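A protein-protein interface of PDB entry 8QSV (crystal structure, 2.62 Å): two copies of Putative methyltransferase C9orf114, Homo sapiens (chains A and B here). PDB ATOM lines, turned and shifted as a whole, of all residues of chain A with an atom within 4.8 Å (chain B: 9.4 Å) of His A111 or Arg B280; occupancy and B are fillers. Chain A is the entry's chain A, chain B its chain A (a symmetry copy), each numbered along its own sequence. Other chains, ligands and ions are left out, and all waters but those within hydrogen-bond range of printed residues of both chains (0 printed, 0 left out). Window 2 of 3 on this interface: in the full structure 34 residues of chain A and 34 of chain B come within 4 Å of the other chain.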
ATOM      1  N   LEU A  80      13.999   3.747   6.226  1.00  0.00           N
ATOM      2  CA  LEU A  80      13.808   5.149   6.554  1.00  0.00           C
ATOM      3  C   LEU A  80      14.620   6.063   5.650  1.00  0.00           C
ATOM      4  O   LEU A  80      14.174   7.159   5.356  1.00  0.00           O
ATOM      5  CB  LEU A  80      14.215   5.369   8.008  1.00  0.00           C
ATOM      6  CG  LEU A  80      13.222   4.825   9.029  1.00  0.00           C
ATOM      7  CD1 LEU A  80      13.803   4.953  10.424  1.00  0.00           C
ATOM      8  CD2 LEU A  80      11.884   5.556   8.915  1.00  0.00           C
ATOM      9  N   GLU A  81      15.831   5.634   5.284  1.00  0.00           N
ATOM     10  CA  GLU A  81      16.748   6.422   4.472  1.00  0.00           C
ATOM     11  C   GLU A  81      16.217   6.496   3.043  1.00  0.00           C
ATOM     12  O   GLU A  81      16.292   7.526   2.388  1.00  0.00           O
ATOM     13  CB  GLU A  81      18.111   5.740   4.571  1.00  0.00           C
ATOM     14  CG  GLU A  81      19.244   6.393   3.797  1.00  0.00           C
ATOM     15  CD  GLU A  81      19.210   6.276   2.288  1.00  0.00           C
ATOM     16  OE1 GLU A  81      18.869   5.174   1.769  1.00  0.00           O
ATOM     17  OE2 GLU A  81      19.537   7.279   1.647  1.00  0.00           O
ATOM     18  N   CYS A  82      15.660   5.387   2.558  1.00  0.00           N
ATOM     19  CA  CYS A  82      15.127   5.373   1.216  1.00  0.00           C
ATOM     20  C   CYS A  82      14.049   6.439   1.091  1.00  0.00           C
ATOM     21  O   CYS A  82      13.116   6.471   1.872  1.00  0.00           O
ATOM     22  CB  CYS A  82      14.584   3.997   0.878  1.00  0.00           C
ATOM     23  SG  CYS A  82      13.897   3.918  -0.793  1.00  0.00           S
ATOM     24  N   PRO A  83      14.106   7.334   0.090  1.00  0.00           N
ATOM     25  CA  PRO A  83      13.019   8.285  -0.140  1.00  0.00           C
ATOM     26  C   PRO A  83      11.723   7.512  -0.315  1.00  0.00           C
ATOM     27  O   PRO A  83      11.774   6.353  -0.695  1.00  0.00           O
ATOM     28  CB  PRO A  83      13.374   9.015  -1.444  1.00  0.00           C
ATOM     29  CG  PRO A  83      14.850   8.718  -1.661  1.00  0.00           C
ATOM     30  CD  PRO A  83      15.170   7.442  -0.908  1.00  0.00           C
ATOM     31  N   ARG A  87      10.228   3.375  -1.654  1.00  0.00           N
ATOM     32  CA  ARG A  87      10.133   2.291  -0.683  1.00  0.00           C
ATOM     33  C   ARG A  87       9.351   1.102  -1.252  1.00  0.00           C
ATOM     34  O   ARG A  87       9.810  -0.035  -1.173  1.00  0.00           O
ATOM     35  CB  ARG A  87       9.463   2.783   0.597  1.00  0.00           C
ATOM     36  CG  ARG A  87      10.166   3.969   1.227  1.00  0.00           C
ATOM     37  CD  ARG A  87       9.784   4.102   2.672  1.00  0.00           C
ATOM     38  NE  ARG A  87      10.732   5.014   3.264  1.00  0.00           N
ATOM     39  CZ  ARG A  87      10.432   6.181   3.804  1.00  0.00           C
ATOM     40  NH1 ARG A  87       9.178   6.585   3.873  1.00  0.00           N
ATOM     41  NH2 ARG A  87      11.395   6.947   4.276  1.00  0.00           N
ATOM     42  N   LEU A 106      12.940  10.916   8.595  1.00  0.00           N
ATOM     43  CA  LEU A 106      14.258  11.543   8.582  1.00  0.00           C
ATOM     44  C   LEU A 106      14.208  12.981   8.071  1.00  0.00           C
ATOM     45  O   LEU A 106      15.071  13.777   8.434  1.00  0.00           O
ATOM     46  CB  LEU A 106      15.210  10.735   7.709  1.00  0.00           C
ATOM     47  CG  LEU A 106      15.554   9.326   8.180  1.00  0.00           C
ATOM     48  CD1 LEU A 106      16.677   8.754   7.340  1.00  0.00           C
ATOM     49  CD2 LEU A 106      15.955   9.324   9.645  1.00  0.00           C
ATOM     50  N   ASP A 107      13.221  13.333   7.238  1.00  0.00           N
ATOM     51  CA  ASP A 107      13.098  14.717   6.796  1.00  0.00           C
ATOM     52  C   ASP A 107      14.449  15.204   6.277  1.00  0.00           C
ATOM     53  O   ASP A 107      14.857  16.331   6.545  1.00  0.00           O
ATOM     54  CB  ASP A 107      12.595  15.672   7.892  1.00  0.00           C
ATOM     55  CG  ASP A 107      11.177  15.415   8.385  1.00  0.00           C
ATOM     56  OD1 ASP A 107      10.534  14.502   7.837  1.00  0.00           O
ATOM     57  OD2 ASP A 107      10.714  16.127   9.330  1.00  0.00           O
ATOM     58  N   SER A 108      15.133  14.340   5.524  1.00  0.00           N
ATOM     59  CA  SER A 108      16.451  14.654   5.003  1.00  0.00           C
ATOM     60  C   SER A 108      16.347  15.264   3.615  1.00  0.00           C
ATOM     61  O   SER A 108      15.352  15.076   2.929  1.00  0.00           O
ATOM     62  CB  SER A 108      17.301  13.438   4.998  1.00  0.00           C
ATOM     63  OG  SER A 108      18.015  13.374   6.234  1.00  0.00           O
ATOM     64  N   PRO A 109      17.366  16.011   3.146  1.00  0.00           N
ATOM     65  CA  PRO A 109      17.274  16.678   1.851  1.00  0.00           C
ATOM     66  C   PRO A 109      16.807  15.821   0.678  1.00  0.00           C
ATOM     67  O   PRO A 109      16.127  16.326  -0.192  1.00  0.00           O
ATOM     68  CB  PRO A 109      18.690  17.238   1.656  1.00  0.00           C
ATOM     69  CG  PRO A 109      19.126  17.558   3.068  1.00  0.00           C
ATOM     70  CD  PRO A 109      18.625  16.349   3.842  1.00  0.00           C
ATOM     71  N   HIS A 110      17.081  14.524   0.654  1.00  0.00           N
ATOM     72  CA  HIS A 110      16.635  13.746  -0.497  1.00  0.00           C
ATOM     73  C   HIS A 110      15.220  13.207  -0.324  1.00  0.00           C
ATOM     74  O   HIS A 110      14.775  12.427  -1.154  1.00  0.00           O
ATOM     75  CB  HIS A 110      17.613  12.626  -0.857  1.00  0.00           C
ATOM     76  CG  HIS A 110      17.865  11.641   0.213  1.00  0.00           C
ATOM     77  ND1 HIS A 110      18.226  12.017   1.486  1.00  0.00           N
ATOM     78  CD2 HIS A 110      17.880  10.312   0.199  1.00  0.00           C
ATOM     79  CE1 HIS A 110      18.427  10.933   2.223  1.00  0.00           C
ATOM     80  NE2 HIS A 110      18.227   9.888   1.463  1.00  0.00           N
ATOM     81  N   HIS A 111      14.524  13.584   0.751  1.00  0.00           N
ATOM     82  CA  HIS A 111      13.113  13.268   0.880  1.00  0.00           C
ATOM     83  C   HIS A 111      12.322  14.546   0.649  1.00  0.00           C
ATOM     84  O   HIS A 111      12.339  15.425   1.501  1.00  0.00           O
ATOM     85  CB  HIS A 111      12.787  12.732   2.264  1.00  0.00           C
ATOM     86  CG  HIS A 111      13.584  11.567   2.690  1.00  0.00           C
ATOM     87  ND1 HIS A 111      13.147  10.806   3.745  1.00  0.00           N
ATOM     88  CD2 HIS A 111      14.710  10.994   2.260  1.00  0.00           C
ATOM     89  CE1 HIS A 111      14.007   9.824   3.953  1.00  0.00           C
ATOM     90  NE2 HIS A 111      14.948   9.905   3.050  1.00  0.00           N
ATOM     91  N   MET A 112      11.700  14.667  -0.530  1.00  0.00           N
ATOM     92  CA  MET A 112      10.843  15.797  -0.847  1.00  0.00           C
ATOM     93  C   MET A 112       9.597  15.224  -1.504  1.00  0.00           C
ATOM     94  O   MET A 112       9.545  14.015  -1.711  1.00  0.00           O
ATOM     95  CB  MET A 112      11.583  16.798  -1.739  1.00  0.00           C
ATOM     96  CG  MET A 112      11.661  16.415  -3.212  1.00  0.00           C
ATOM     97  SD  MET A 112      13.403  15.677  -3.698  1.00  0.00           S
ATOM     98  CE  MET A 112      12.952  13.797  -3.701  1.00  0.00           C
ATOM     99  N   ARG A 113       8.609  16.084  -1.782  1.00  0.00           N
ATOM    100  CA  ARG A 113       7.459  15.695  -2.582  1.00  0.00           C
ATOM    101  C   ARG A 113       7.679  16.209  -4.004  1.00  0.00           C
ATOM    102  O   ARG A 113       8.505  17.098  -4.201  1.00  0.00           O
ATOM    103  CB  ARG A 113       6.160  16.243  -1.974  1.00  0.00           C
ATOM    104  CG  ARG A 113       4.896  15.630  -2.571  1.00  0.00           C
ATOM    105  CD  ARG A 113       3.613  16.443  -2.437  1.00  0.00           C
ATOM    106  NE  ARG A 113       2.703  16.218  -3.564  1.00  0.00           N
ATOM    107  CZ  ARG A 113       2.163  15.043  -3.905  1.00  0.00           C
ATOM    108  NH1 ARG A 113       2.361  13.980  -3.144  1.00  0.00           N
ATOM    109  NH2 ARG A 113       1.418  14.938  -4.999  1.00  0.00           N
ATOM    110  N   GLU B 222      16.871  26.416  15.638  1.00  0.00           N
ATOM    111  CA  GLU B 222      17.649  26.374  14.415  1.00  0.00           C
ATOM    112  C   GLU B 222      18.017  27.779  13.937  1.00  0.00           C
ATOM    113  O   GLU B 222      19.035  27.924  13.272  1.00  0.00           O
ATOM    114  CB  GLU B 222      16.910  25.588  13.325  1.00  0.00           C
ATOM    115  CG  GLU B 222      15.535  26.133  12.975  1.00  0.00           C
ATOM    116  CD  GLU B 222      14.581  25.099  12.398  1.00  0.00           C
ATOM    117  OE1 GLU B 222      13.655  24.664  13.131  1.00  0.00           O
ATOM    118  OE2 GLU B 222      14.756  24.738  11.218  1.00  0.00           O
ATOM    119  N   ARG B 223      17.224  28.817  14.246  1.00  0.00           N
ATOM    120  CA  ARG B 223      17.557  30.146  13.735  1.00  0.00           C
ATOM    121  C   ARG B 223      18.204  30.989  14.838  1.00  0.00           C
ATOM    122  O   ARG B 223      18.293  32.205  14.721  1.00  0.00           O
ATOM    123  CB  ARG B 223      16.380  30.812  12.995  1.00  0.00           C
ATOM    124  CG  ARG B 223      15.042  30.781  13.715  1.00  0.00           C
ATOM    125  CD  ARG B 223      13.913  31.413  12.914  1.00  0.00           C
ATOM    126  NE  ARG B 223      13.221  30.425  12.106  1.00  0.00           N
ATOM    127  CZ  ARG B 223      12.338  29.552  12.581  1.00  0.00           C
ATOM    128  NH1 ARG B 223      11.737  29.777  13.735  1.00  0.00           N
ATOM    129  NH2 ARG B 223      12.018  28.482  11.873  1.00  0.00           N
ATOM    130  N   LEU B 245       6.528  21.773  18.774  1.00  0.00           N
ATOM    131  CA  LEU B 245       6.501  21.567  17.333  1.00  0.00           C
ATOM    132  C   LEU B 245       6.581  22.884  16.570  1.00  0.00           C
ATOM    133  O   LEU B 245       7.199  22.963  15.523  1.00  0.00           O
ATOM    134  CB  LEU B 245       5.206  20.806  17.013  1.00  0.00           C
ATOM    135  CG  LEU B 245       5.005  20.392  15.555  1.00  0.00           C
ATOM    136  CD1 LEU B 245       6.287  19.867  14.952  1.00  0.00           C
ATOM    137  CD2 LEU B 245       3.916  19.331  15.435  1.00  0.00           C
ATOM    138  N   ASN B 272      21.513  27.887  18.173  1.00  0.00           N
ATOM    139  CA  ASN B 272      21.414  26.666  17.381  1.00  0.00           C
ATOM    140  C   ASN B 272      22.532  25.728  17.817  1.00  0.00           C
ATOM    141  O   ASN B 272      23.707  26.063  17.682  1.00  0.00           O
ATOM    142  CB  ASN B 272      21.523  26.928  15.874  1.00  0.00           C
ATOM    143  CG  ASN B 272      21.573  25.665  15.026  1.00  0.00           C
ATOM    144  OD1 ASN B 272      21.946  24.596  15.503  1.00  0.00           O
ATOM    145  ND2 ASN B 272      21.178  25.760  13.766  1.00  0.00           N
ATOM    146  N   CYS B 274      22.964  22.423  16.836  1.00  0.00           N
ATOM    147  CA  CYS B 274      23.399  21.437  15.869  1.00  0.00           C
ATOM    148  C   CYS B 274      23.639  22.103  14.516  1.00  0.00           C
ATOM    149  O   CYS B 274      22.761  22.157  13.652  1.00  0.00           O
ATOM    150  CB  CYS B 274      22.350  20.344  15.790  1.00  0.00           C
ATOM    151  SG  CYS B 274      22.937  18.894  14.886  1.00  0.00           S
ATOM    152  N   GLY B 276      24.502  22.720  10.720  1.00  0.00           N
ATOM    153  CA  GLY B 276      24.466  21.859   9.541  1.00  0.00           C
ATOM    154  C   GLY B 276      23.742  20.519   9.737  1.00  0.00           C
ATOM    155  O   GLY B 276      24.212  19.459   9.328  1.00  0.00           O
ATOM    156  N   GLN B 277      22.559  20.587  10.324  1.00  0.00           N
ATOM    157  CA  GLN B 277      21.764  19.422  10.635  1.00  0.00           C
ATOM    158  C   GLN B 277      21.263  18.790   9.346  1.00  0.00           C
ATOM    159  O   GLN B 277      20.851  19.495   8.430  1.00  0.00           O
ATOM    160  CB  GLN B 277      20.608  19.846  11.544  1.00  0.00           C
ATOM    161  CG  GLN B 277      19.548  20.677  10.841  1.00  0.00           C
ATOM    162  CD  GLN B 277      18.541  21.250  11.812  1.00  0.00           C
ATOM    163  OE1 GLN B 277      18.847  22.090  12.655  1.00  0.00           O
ATOM    164  NE2 GLN B 277      17.309  20.796  11.685  1.00  0.00           N
ATOM    165  N   GLY B 278      21.288  17.455   9.305  1.00  0.00           N
ATOM    166  CA  GLY B 278      20.949  16.718   8.103  1.00  0.00           C
ATOM    167  C   GLY B 278      19.473  16.352   8.047  1.00  0.00           C
ATOM    168  O   GLY B 278      19.017  15.777   7.076  1.00  0.00           O
ATOM    169  N   SER B 279      18.727  16.675   9.101  1.00  0.00           N
ATOM    170  CA  SER B 279      17.284  16.529   9.093  1.00  0.00           C
ATOM    171  C   SER B 279      16.705  17.924   9.167  1.00  0.00           C
ATOM    172  O   SER B 279      17.285  18.766   9.829  1.00  0.00           O
ATOM    173  CB  SER B 279      16.786  15.692  10.252  1.00  0.00           C
ATOM    174  OG  SER B 279      15.366  15.551  10.212  1.00  0.00           O
ATOM    175  N   ARG B 280      15.551  18.126   8.524  1.00  0.00           N
ATOM    176  CA  ARG B 280      14.859  19.405   8.499  1.00  0.00           C
ATOM    177  C   ARG B 280      14.375  19.748   9.904  1.00  0.00           C
ATOM    178  O   ARG B 280      14.155  20.912  10.201  1.00  0.00           O
ATOM    179  CB  ARG B 280      13.671  19.331   7.535  1.00  0.00           C
ATOM    180  CG  ARG B 280      13.590  20.445   6.500  1.00  0.00           C
ATOM    181  CD  ARG B 280      14.339  20.211   5.188  1.00  0.00           C
ATOM    182  NE  ARG B 280      14.205  18.927   4.477  1.00  0.00           N
ATOM    183  CZ  ARG B 280      13.067  18.286   4.184  1.00  0.00           C
ATOM    184  NH1 ARG B 280      11.918  18.683   4.695  1.00  0.00           N
ATOM    185  NH2 ARG B 280      13.090  17.204   3.423  1.00  0.00           N
ATOM    186  N   THR B 281      14.175  18.729  10.754  1.00  0.00           N
ATOM    187  CA  THR B 281      13.698  18.944  12.111  1.00  0.00           C
ATOM    188  C   THR B 281      14.452  18.092  13.123  1.00  0.00           C
ATOM    189  O   THR B 281      14.914  17.014  12.815  1.00  0.00           O
ATOM    190  CB  THR B 281      12.201  18.643  12.264  1.00  0.00           C
ATOM    191  OG1 THR B 281      11.961  17.390  11.619  1.00  0.00           O
ATOM    192  CG2 THR B 281      11.320  19.755  11.712  1.00  0.00           C
ATOM    193  N   ILE B 282      14.587  18.643  14.320  1.00  0.00           N
ATOM    194  CA  ILE B 282      15.082  17.963  15.494  1.00  0.00           C
ATOM    195  C   ILE B 282      13.970  18.026  16.514  1.00  0.00           C
ATOM    196  O   ILE B 282      13.546  19.099  16.834  1.00  0.00           O
ATOM    197  CB  ILE B 282      16.326  18.671  16.045  1.00  0.00           C
ATOM    198  CG1 ILE B 282      17.423  18.728  14.979  1.00  0.00           C
ATOM    199  CG2 ILE B 282      16.812  18.006  17.331  1.00  0.00           C
ATOM    200  CD1 ILE B 282      18.590  19.593  15.369  1.00  0.00           C
ATOM    201  N   ARG B 283      13.500  16.884  17.003  1.00  0.00           N
ATOM    202  CA  ARG B 283      12.388  16.850  17.931  1.00  0.00           C
ATOM    203  C   ARG B 283      12.834  17.380  19.295  1.00  0.00           C
ATOM    204  O   ARG B 283      14.008  17.429  19.605  1.00  0.00           O
ATOM    205  CB  ARG B 283      11.885  15.411  18.066  1.00  0.00           C
ATOM    206  CG  ARG B 283      11.044  14.858  16.920  1.00  0.00           C
ATOM    207  CD  ARG B 283      10.489  13.535  17.480  1.00  0.00           C
ATOM    208  NE  ARG B 283       9.528  12.828  16.664  1.00  0.00           N
ATOM    209  CZ  ARG B 283       9.634  11.540  16.313  1.00  0.00           C
ATOM    210  NH1 ARG B 283      10.549  10.775  16.879  1.00  0.00           N
ATOM    211  NH2 ARG B 283       8.792  10.991  15.440  1.00  0.00           N
ATOM    212  N   GLU B 286      14.944  15.094  21.371  1.00  0.00           N
ATOM    213  CA  GLU B 286      16.244  14.938  20.746  1.00  0.00           C
ATOM    214  C   GLU B 286      17.083  16.186  20.996  1.00  0.00           C
ATOM    215  O   GLU B 286      18.278  16.111  21.310  1.00  0.00           O
ATOM    216  CB  GLU B 286      16.108  14.775  19.227  1.00  0.00           C
ATOM    217  CG  GLU B 286      15.463  13.481  18.779  1.00  0.00           C
ATOM    218  CD  GLU B 286      15.074  13.450  17.305  1.00  0.00           C
ATOM    219  OE1 GLU B 286      14.996  14.546  16.747  1.00  0.00           O
ATOM    220  OE2 GLU B 286      14.822  12.335  16.715  1.00  0.00           O
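Of the 14 printed residues of chain B, 4 touch a printed residue of chain A. Printed residues of chain B that touch a printed residue of chain A: Gly B278, Ser B279, Arg B280 and Thr B281. Among the printed residues, 8 pairs touch across the chains. Among the printed residues, no Asp or Glu carboxylate lies within 4 Å of a Lys or Arg side-chain nitrogen of the other chain.
Of chain B, only Arg B280 comes within 4 Å of His A111. No residue of chain B comes within 4 Å of Met A112. Printed residues of chain A within 4 Å of Gly B278: Ser A108 and Pro A109. Of the printed residues of chain A, Thr B281 touches Asp A107. The nearest residue of chain B that does not touch His A111 is Gly B278 (8.0 Å). The nearest residue of chain A that does not touch Arg B280 is Leu A106 (4.4 Å). The nearest printed residue of chain B that does not touch Pro A109 is Arg B280 (4.4 Å).
No position is printed for both chains. Of the 8 pairs that touch across the chains among the printed residues, none has its exchanged pair printed and touching as well.
Ser B279 touches Asp A107 (CA to O, 3.5 Å). Pro A109 touches Gly B278.
O of Glu A81 lies within hydrogen-bond range of NE2 of His A111 (2.8 Å). The side-chain amide nitrogen (NE2) of Gln B277 sits at hydrogen-bond distance from the backbone carbonyl oxygen (O) of Ser B279 (2.8 Å). O of Arg B280 lies within hydrogen-bond range of NE2 of Gln B277 (3.5 Å). The side-chain hydroxyl (OG) of Ser B279 is in hydrogen-bond range of the backbone carbonyl oxygen (O) of Thr B281 (3.0 Å).
O of Leu A106 sits at hydrogen-bond distance from OG of Ser B279 (2.5 Å). N of Arg B280 lies within hydrogen-bond range of O of Asp A107 (2.8 Å). The side-chain carboxylate (OD2) of Asp A107 lies within hydrogen-bond range of the side-chain hydroxyl (OG1) of Thr B281, at 2.9 Å. The side-chain hydroxyl (OG) of Ser A108 is in hydrogen-bond range of the backbone carbonyl oxygen (O) of Gly B278 (2.7 Å). The backbone carbonyl oxygen of Ser A108 sits at hydrogen-bond distance from the guanidinium group of Arg B280 (3.1 Å). NH2 of Arg B280 is in hydrogen-bond range of O of His A111 (2.7 Å).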
